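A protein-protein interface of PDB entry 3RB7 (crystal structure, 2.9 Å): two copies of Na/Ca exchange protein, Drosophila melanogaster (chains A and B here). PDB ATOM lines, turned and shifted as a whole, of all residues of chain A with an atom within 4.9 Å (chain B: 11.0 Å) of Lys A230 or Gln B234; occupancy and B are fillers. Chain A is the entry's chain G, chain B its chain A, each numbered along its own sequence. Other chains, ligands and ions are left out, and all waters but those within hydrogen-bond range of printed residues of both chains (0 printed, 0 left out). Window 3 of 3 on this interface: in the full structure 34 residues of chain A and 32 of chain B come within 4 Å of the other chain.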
ATOM      1  N   LYS A 226     -20.009 -32.373  28.668  1.00  0.00           N
ATOM      2  CA  LYS A 226     -20.251 -31.243  27.776  1.00  0.00           C
ATOM      3  C   LYS A 226     -20.579 -31.718  26.365  1.00  0.00           C
ATOM      4  O   LYS A 226     -21.069 -30.947  25.538  1.00  0.00           O
ATOM      5  CB  LYS A 226     -19.097 -30.231  27.801  1.00  0.00           C
ATOM      6  CG  LYS A 226     -17.730 -30.804  28.100  1.00  0.00           C
ATOM      7  CD  LYS A 226     -16.685 -29.682  28.208  1.00  0.00           C
ATOM      8  CE  LYS A 226     -15.988 -29.341  26.865  1.00  0.00           C
ATOM      9  NZ  LYS A 226     -14.835 -30.239  26.502  1.00  0.00           N
ATOM     10  N   GLU A 227     -20.302 -32.997  26.116  1.00  0.00           N
ATOM     11  CA  GLU A 227     -20.769 -33.716  24.932  1.00  0.00           C
ATOM     12  C   GLU A 227     -22.295 -33.793  24.918  1.00  0.00           C
ATOM     13  O   GLU A 227     -22.956 -33.306  23.995  1.00  0.00           O
ATOM     14  CB  GLU A 227     -20.192 -35.137  24.934  1.00  0.00           C
ATOM     15  CG  GLU A 227     -20.993 -36.151  24.142  1.00  0.00           C
ATOM     16  CD  GLU A 227     -20.398 -36.431  22.775  1.00  0.00           C
ATOM     17  OE1 GLU A 227     -19.441 -37.235  22.712  1.00  0.00           O
ATOM     18  OE2 GLU A 227     -20.894 -35.867  21.768  1.00  0.00           O
ATOM     19  N   VAL A 228     -22.847 -34.413  25.957  1.00  0.00           N
ATOM     20  CA  VAL A 228     -24.290 -34.568  26.080  1.00  0.00           C
ATOM     21  C   VAL A 228     -24.970 -33.223  26.364  1.00  0.00           C
ATOM     22  O   VAL A 228     -26.097 -32.985  25.941  1.00  0.00           O
ATOM     23  CB  VAL A 228     -24.647 -35.611  27.165  1.00  0.00           C
ATOM     24  CG1 VAL A 228     -24.367 -35.065  28.538  1.00  0.00           C
ATOM     25  CG2 VAL A 228     -26.092 -36.010  27.060  1.00  0.00           C
ATOM     26  N   GLU A 229     -24.275 -32.337  27.067  1.00  0.00           N
ATOM     27  CA  GLU A 229     -24.797 -31.004  27.334  1.00  0.00           C
ATOM     28  C   GLU A 229     -25.055 -30.225  26.042  1.00  0.00           C
ATOM     29  O   GLU A 229     -25.487 -29.073  26.077  1.00  0.00           O
ATOM     30  CB  GLU A 229     -23.831 -30.220  28.226  1.00  0.00           C
ATOM     31  CG  GLU A 229     -23.641 -30.811  29.617  1.00  0.00           C
ATOM     32  CD  GLU A 229     -23.419 -29.741  30.674  1.00  0.00           C
ATOM     33  OE1 GLU A 229     -23.887 -28.603  30.458  1.00  0.00           O
ATOM     34  OE2 GLU A 229     -22.784 -30.028  31.713  1.00  0.00           O
ATOM     35  N   LYS A 230     -24.768 -30.856  24.904  1.00  0.00           N
ATOM     36  CA  LYS A 230     -25.041 -30.273  23.594  1.00  0.00           C
ATOM     37  C   LYS A 230     -26.485 -30.567  23.200  1.00  0.00           C
ATOM     38  O   LYS A 230     -27.124 -29.789  22.487  1.00  0.00           O
ATOM     39  CB  LYS A 230     -24.092 -30.870  22.552  1.00  0.00           C
ATOM     40  CG  LYS A 230     -22.622 -30.749  22.915  1.00  0.00           C
ATOM     41  CD  LYS A 230     -21.890 -29.697  22.087  1.00  0.00           C
ATOM     42  CE  LYS A 230     -21.210 -30.333  20.889  1.00  0.00           C
ATOM     43  NZ  LYS A 230     -20.616 -31.646  21.280  1.00  0.00           N
ATOM     44  N   LYS A 231     -26.986 -31.704  23.680  1.00  0.00           N
ATOM     45  CA  LYS A 231     -28.322 -32.179  23.348  1.00  0.00           C
ATOM     46  C   LYS A 231     -29.399 -31.229  23.831  1.00  0.00           C
ATOM     47  O   LYS A 231     -29.275 -30.654  24.916  1.00  0.00           O
ATOM     48  CB  LYS A 231     -28.579 -33.541  23.997  1.00  0.00           C
ATOM     49  CG  LYS A 231     -28.135 -34.749  23.199  1.00  0.00           C
ATOM     50  CD  LYS A 231     -27.818 -35.873  24.157  1.00  0.00           C
ATOM     51  CE  LYS A 231     -27.809 -37.229  23.492  1.00  0.00           C
ATOM     52  NZ  LYS A 231     -29.157 -37.874  23.521  1.00  0.00           N
ATOM     53  N   PRO A 232     -30.461 -31.065  23.023  1.00  0.00           N
ATOM     54  CA  PRO A 232     -31.714 -30.507  23.528  1.00  0.00           C
ATOM     55  C   PRO A 232     -32.189 -31.384  24.678  1.00  0.00           C
ATOM     56  O   PRO A 232     -32.287 -32.608  24.518  1.00  0.00           O
ATOM     57  CB  PRO A 232     -32.659 -30.641  22.329  1.00  0.00           C
ATOM     58  CG  PRO A 232     -31.977 -31.626  21.417  1.00  0.00           C
ATOM     59  CD  PRO A 232     -30.543 -31.319  21.578  1.00  0.00           C
ATOM     60  N   VAL B 228     -39.003 -25.321  26.925  1.00  0.00           N
ATOM     61  CA  VAL B 228     -37.608 -25.146  27.318  1.00  0.00           C
ATOM     62  C   VAL B 228     -36.796 -26.389  26.929  1.00  0.00           C
ATOM     63  O   VAL B 228     -35.679 -26.269  26.414  1.00  0.00           O
ATOM     64  CB  VAL B 228     -37.448 -24.812  28.841  1.00  0.00           C
ATOM     65  CG1 VAL B 228     -37.441 -26.072  29.680  1.00  0.00           C
ATOM     66  CG2 VAL B 228     -36.169 -24.021  29.102  1.00  0.00           C
ATOM     67  N   GLU B 229     -37.368 -27.573  27.150  1.00  0.00           N
ATOM     68  CA  GLU B 229     -36.700 -28.831  26.804  1.00  0.00           C
ATOM     69  C   GLU B 229     -36.331 -28.861  25.321  1.00  0.00           C
ATOM     70  O   GLU B 229     -35.651 -29.774  24.859  1.00  0.00           O
ATOM     71  CB  GLU B 229     -37.577 -30.030  27.163  1.00  0.00           C
ATOM     72  CG  GLU B 229     -38.027 -30.064  28.624  1.00  0.00           C
ATOM     73  CD  GLU B 229     -39.034 -31.175  28.899  1.00  0.00           C
ATOM     74  OE1 GLU B 229     -39.559 -31.752  27.922  1.00  0.00           O
ATOM     75  OE2 GLU B 229     -39.301 -31.476  30.086  1.00  0.00           O
ATOM     76  N   LYS B 230     -36.802 -27.851  24.592  1.00  0.00           N
ATOM     77  CA  LYS B 230     -36.378 -27.582  23.222  1.00  0.00           C
ATOM     78  C   LYS B 230     -34.894 -27.193  23.205  1.00  0.00           C
ATOM     79  O   LYS B 230     -34.137 -27.628  22.336  1.00  0.00           O
ATOM     80  CB  LYS B 230     -37.218 -26.445  22.623  1.00  0.00           C
ATOM     81  CG  LYS B 230     -38.719 -26.697  22.595  1.00  0.00           C
ATOM     82  CD  LYS B 230     -39.105 -27.681  21.502  1.00  0.00           C
ATOM     83  CE  LYS B 230     -39.470 -26.975  20.208  1.00  0.00           C
ATOM     84  NZ  LYS B 230     -40.755 -26.240  20.361  1.00  0.00           N
ATOM     85  N   LYS B 231     -34.491 -26.380  24.181  1.00  0.00           N
ATOM     86  CA  LYS B 231     -33.124 -25.886  24.283  1.00  0.00           C
ATOM     87  C   LYS B 231     -32.163 -26.960  24.773  1.00  0.00           C
ATOM     88  O   LYS B 231     -32.459 -27.666  25.729  1.00  0.00           O
ATOM     89  CB  LYS B 231     -33.066 -24.706  25.250  1.00  0.00           C
ATOM     90  CG  LYS B 231     -34.088 -23.616  25.002  1.00  0.00           C
ATOM     91  CD  LYS B 231     -33.891 -22.472  25.993  1.00  0.00           C
ATOM     92  CE  LYS B 231     -34.775 -21.263  25.676  1.00  0.00           C
ATOM     93  NZ  LYS B 231     -34.552 -20.106  26.606  1.00  0.00           N
ATOM     94  N   PRO B 232     -30.996 -27.081  24.125  1.00  0.00           N
ATOM     95  CA  PRO B 232     -29.954 -27.990  24.603  1.00  0.00           C
ATOM     96  C   PRO B 232     -29.514 -27.606  25.996  1.00  0.00           C
ATOM     97  O   PRO B 232     -29.318 -26.418  26.249  1.00  0.00           O
ATOM     98  CB  PRO B 232     -28.795 -27.739  23.638  1.00  0.00           C
ATOM     99  CG  PRO B 232     -29.415 -27.186  22.431  1.00  0.00           C
ATOM    100  CD  PRO B 232     -30.592 -26.385  22.895  1.00  0.00           C
ATOM    101  N   VAL B 233     -29.370 -28.596  26.874  1.00  0.00           N
ATOM    102  CA  VAL B 233     -28.828 -28.405  28.221  1.00  0.00           C
ATOM    103  C   VAL B 233     -27.930 -27.176  28.284  1.00  0.00           C
ATOM    104  O   VAL B 233     -28.110 -26.276  29.111  1.00  0.00           O
ATOM    105  CB  VAL B 233     -27.978 -29.621  28.626  1.00  0.00           C
ATOM    106  CG1 VAL B 233     -27.339 -29.400  29.979  1.00  0.00           C
ATOM    107  CG2 VAL B 233     -28.816 -30.887  28.615  1.00  0.00           C
ATOM    108  N   GLN B 234     -26.955 -27.177  27.384  1.00  0.00           N
ATOM    109  CA  GLN B 234     -26.005 -26.101  27.197  1.00  0.00           C
ATOM    110  C   GLN B 234     -26.612 -24.723  27.399  1.00  0.00           C
ATOM    111  O   GLN B 234     -26.160 -23.966  28.255  1.00  0.00           O
ATOM    112  CB  GLN B 234     -25.479 -26.184  25.776  1.00  0.00           C
ATOM    113  CG  GLN B 234     -23.993 -26.211  25.668  1.00  0.00           C
ATOM    114  CD  GLN B 234     -23.567 -26.917  24.421  1.00  0.00           C
ATOM    115  OE1 GLN B 234     -24.055 -26.619  23.326  1.00  0.00           O
ATOM    116  NE2 GLN B 234     -22.667 -27.881  24.570  1.00  0.00           N
ATOM    117  N   ASP B 235     -27.623 -24.394  26.597  1.00  0.00           N
ATOM    118  CA  ASP B 235     -28.175 -23.040  26.580  1.00  0.00           C
ATOM    119  C   ASP B 235     -29.353 -22.884  27.547  1.00  0.00           C
ATOM    120  O   ASP B 235     -30.490 -22.647  27.120  1.00  0.00           O
ATOM    121  CB  ASP B 235     -28.626 -22.634  25.164  1.00  0.00           C
ATOM    122  CG  ASP B 235     -27.999 -23.483  24.069  1.00  0.00           C
ATOM    123  OD1 ASP B 235     -26.773 -23.728  24.113  1.00  0.00           O
ATOM    124  OD2 ASP B 235     -28.742 -23.897  23.150  1.00  0.00           O
ATOM    125  N   LEU B 236     -29.082 -23.013  28.847  1.00  0.00           N
ATOM    126  CA  LEU B 236     -30.112 -22.831  29.876  1.00  0.00           C
ATOM    127  C   LEU B 236     -29.727 -21.769  30.920  1.00  0.00           C
ATOM    128  O   LEU B 236     -28.623 -21.807  31.469  1.00  0.00           O
ATOM    129  CB  LEU B 236     -30.428 -24.171  30.563  1.00  0.00           C
ATOM    130  CG  LEU B 236     -31.456 -25.097  29.896  1.00  0.00           C
ATOM    131  CD1 LEU B 236     -31.106 -25.380  28.452  1.00  0.00           C
ATOM    132  CD2 LEU B 236     -31.581 -26.404  30.643  1.00  0.00           C
ATOM    133  N   THR B 237     -30.630 -20.828  31.198  1.00  0.00           N
ATOM    134  CA  THR B 237     -30.388 -19.871  32.283  1.00  0.00           C
ATOM    135  C   THR B 237     -30.454 -20.523  33.651  1.00  0.00           C
ATOM    136  O   THR B 237     -30.795 -21.695  33.782  1.00  0.00           O
ATOM    137  CB  THR B 237     -31.397 -18.705  32.317  1.00  0.00           C
ATOM    138  OG1 THR B 237     -32.624 -19.099  31.691  1.00  0.00           O
ATOM    139  CG2 THR B 237     -30.822 -17.476  31.633  1.00  0.00           C
ATOM    140  N   GLU B 238     -30.130 -19.738  34.671  1.00  0.00           N
ATOM    141  CA  GLU B 238     -30.300 -20.166  36.047  1.00  0.00           C
ATOM    142  C   GLU B 238     -31.791 -20.347  36.301  1.00  0.00           C
ATOM    143  O   GLU B 238     -32.243 -21.422  36.699  1.00  0.00           O
ATOM    144  CB  GLU B 238     -29.717 -19.109  36.992  1.00  0.00           C
ATOM    145  CG  GLU B 238     -29.660 -19.513  38.465  1.00  0.00           C
ATOM    146  CD  GLU B 238     -28.662 -20.627  38.742  1.00  0.00           C
ATOM    147  OE1 GLU B 238     -28.684 -21.652  38.020  1.00  0.00           O
ATOM    148  OE2 GLU B 238     -27.867 -20.479  39.697  1.00  0.00           O
ATOM    149  N   ASP B 240     -34.229 -20.645  34.102  1.00  0.00           N
ATOM    150  CA  ASP B 240     -34.652 -21.775  33.269  1.00  0.00           C
ATOM    151  C   ASP B 240     -34.156 -23.108  33.814  1.00  0.00           C
ATOM    152  O   ASP B 240     -34.834 -24.134  33.699  1.00  0.00           O
ATOM    153  CB  ASP B 240     -34.141 -21.606  31.833  1.00  0.00           C
ATOM    154  CG  ASP B 240     -35.048 -20.727  30.987  1.00  0.00           C
ATOM    155  OD1 ASP B 240     -36.270 -20.709  31.254  1.00  0.00           O
ATOM    156  OD2 ASP B 240     -34.544 -20.059  30.055  1.00  0.00           O
ATOM    157  N   ARG B 241     -32.960 -23.084  34.391  1.00  0.00           N
ATOM    158  CA  ARG B 241     -32.332 -24.282  34.905  1.00  0.00           C
ATOM    159  C   ARG B 241     -33.183 -24.826  36.037  1.00  0.00           C
ATOM    160  O   ARG B 241     -33.381 -26.034  36.154  1.00  0.00           O
ATOM    161  CB  ARG B 241     -30.939 -23.954  35.420  1.00  0.00           C
ATOM    162  CG  ARG B 241     -29.872 -24.942  35.003  1.00  0.00           C
ATOM    163  CD  ARG B 241     -28.676 -24.909  35.957  1.00  0.00           C
ATOM    164  NE  ARG B 241     -28.822 -25.835  37.087  1.00  0.00           N
ATOM    165  CZ  ARG B 241     -29.098 -25.474  38.341  1.00  0.00           C
ATOM    166  NH1 ARG B 241     -29.260 -24.192  38.657  1.00  0.00           N
ATOM    167  NH2 ARG B 241     -29.205 -26.402  39.286  1.00  0.00           N
ATOM    168  N   LEU B 244     -36.630 -26.445  35.548  1.00  0.00           N
ATOM    169  CA  LEU B 244     -36.482 -27.854  35.201  1.00  0.00           C
ATOM    170  C   LEU B 244     -36.172 -28.721  36.418  1.00  0.00           C
ATOM    171  O   LEU B 244     -36.202 -29.954  36.347  1.00  0.00           O
ATOM    172  CB  LEU B 244     -35.396 -28.014  34.144  1.00  0.00           C
ATOM    173  CG  LEU B 244     -35.802 -27.463  32.780  1.00  0.00           C
ATOM    174  CD1 LEU B 244     -34.583 -27.053  31.981  1.00  0.00           C
ATOM    175  CD2 LEU B 244     -36.649 -28.487  32.026  1.00  0.00           C
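The backbone NH (N) of Val B233 is in hydrogen-bond range of the backbone carbonyl oxygen (O) of Lys A231 (2.8 Å).
The backbone NH of Gln B234 sits at hydrogen-bond distance from the backbone carbonyl oxygen of Glu A229, 2.7 Å away.
NZ of Lys B231 lies within salt-bridge range of OD2 of Asp B240 (3.4 Å).
Lys A226 touches Gln B234.
Glu A229 touches Val B233.
CB of Pro B232 touches O of Lys A230 (2.9 Å).
Lys A230 touches Gln B234 (CD to NE2, 3.2 Å).
Lys A231 touches Pro B232 (O to CA, 2.8 Å).
Pro A232 touches Glu B229.
Pro A232 touches Lys B230 (CB to O, 3.4 Å).
CA of Pro A232 touches O of Lys B231, 3.7 Å away.
Pro B232 touches Pro A232 (CA to CA, 3.3 Å).
Printed residues of chain B within 4 Å of Lys A226: Gln B234 (3.6 Å).
No residue of chain B comes within 4 Å of Glu A227.
Glu A229 touches two residues of chain B.
Of chain B, only Pro B232 (2.9 Å) and Gln B234 (3.2 Å) come within 4 Å of Lys A230.
Of the printed residues of chain B, Lys A231 touches Pro B232 (2.8 Å) and Val B233 (2.8 Å).
Pro A232 touches just these residues of chain B: Glu B229 (3.8 Å), Lys B230 (3.4 Å), Lys B231 (3.7 Å) and Pro B232 (3.3 Å).
Val B228 touches none of the printed residues of chain A.
Of the printed residues of chain A, Lys B230 touches Pro A232.
Of the printed residues of chain A, Pro B232 touches Lys A230, Lys A231 and Pro A232.
Of the printed residues of chain A, Gln B234 touches Lys A226, Glu A229 and Lys A230.
Leu B236 touches none of the printed residues of chain A.
The nearest printed residue of chain A that does not touch Gln B234 is Lys A231 (4.9 Å).
The nearest printed residue of chain A that does not touch Glu B229 is Lys A231 (6.4 Å).
Printed residues of chain A that touch a printed residue of chain B: Lys A226, Glu A229, Lys A230, Lys A231 and Pro A232.
Hydrophobic or aromatic side chains of chain A that line the printed part of chain B: Pro A232.
Printed residues of chain B that touch a printed residue of chain A: Glu B229, Lys B230, Lys B231, Pro B232, Val B233 and Gln B234.
Hydrophobic or aromatic side chains of chain B that line the printed part of chain A: Pro B232 and Val B233.
Along chain B the printed residues that touch a printed residue of chain A span positions 229 to 234.
Among the printed residues, 11 pairs touch across the chains.
Among the printed residues, no Asp or Glu carboxylate lies within 4 Å of a Lys or Arg side-chain nitrogen of the other chain.
Lys A230 touches Pro B232, and with the chains exchanged Pro A232 touches Lys B230.
Lys A231 touches Pro B232, and with the chains exchanged Pro A232 touches Lys B231.
Pro A232 touches Glu B229, but with the chains exchanged Glu A229 does not touch Pro B232 (4.3 Å).
Pro B232 touches its own counterpart, Pro A232.
Positions printed for both chains: 228, 229, 230, 231 and 232.
Of the 11 pairs that touch across the chains among the printed residues, 5 have their exchanged pair printed and touching as well.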
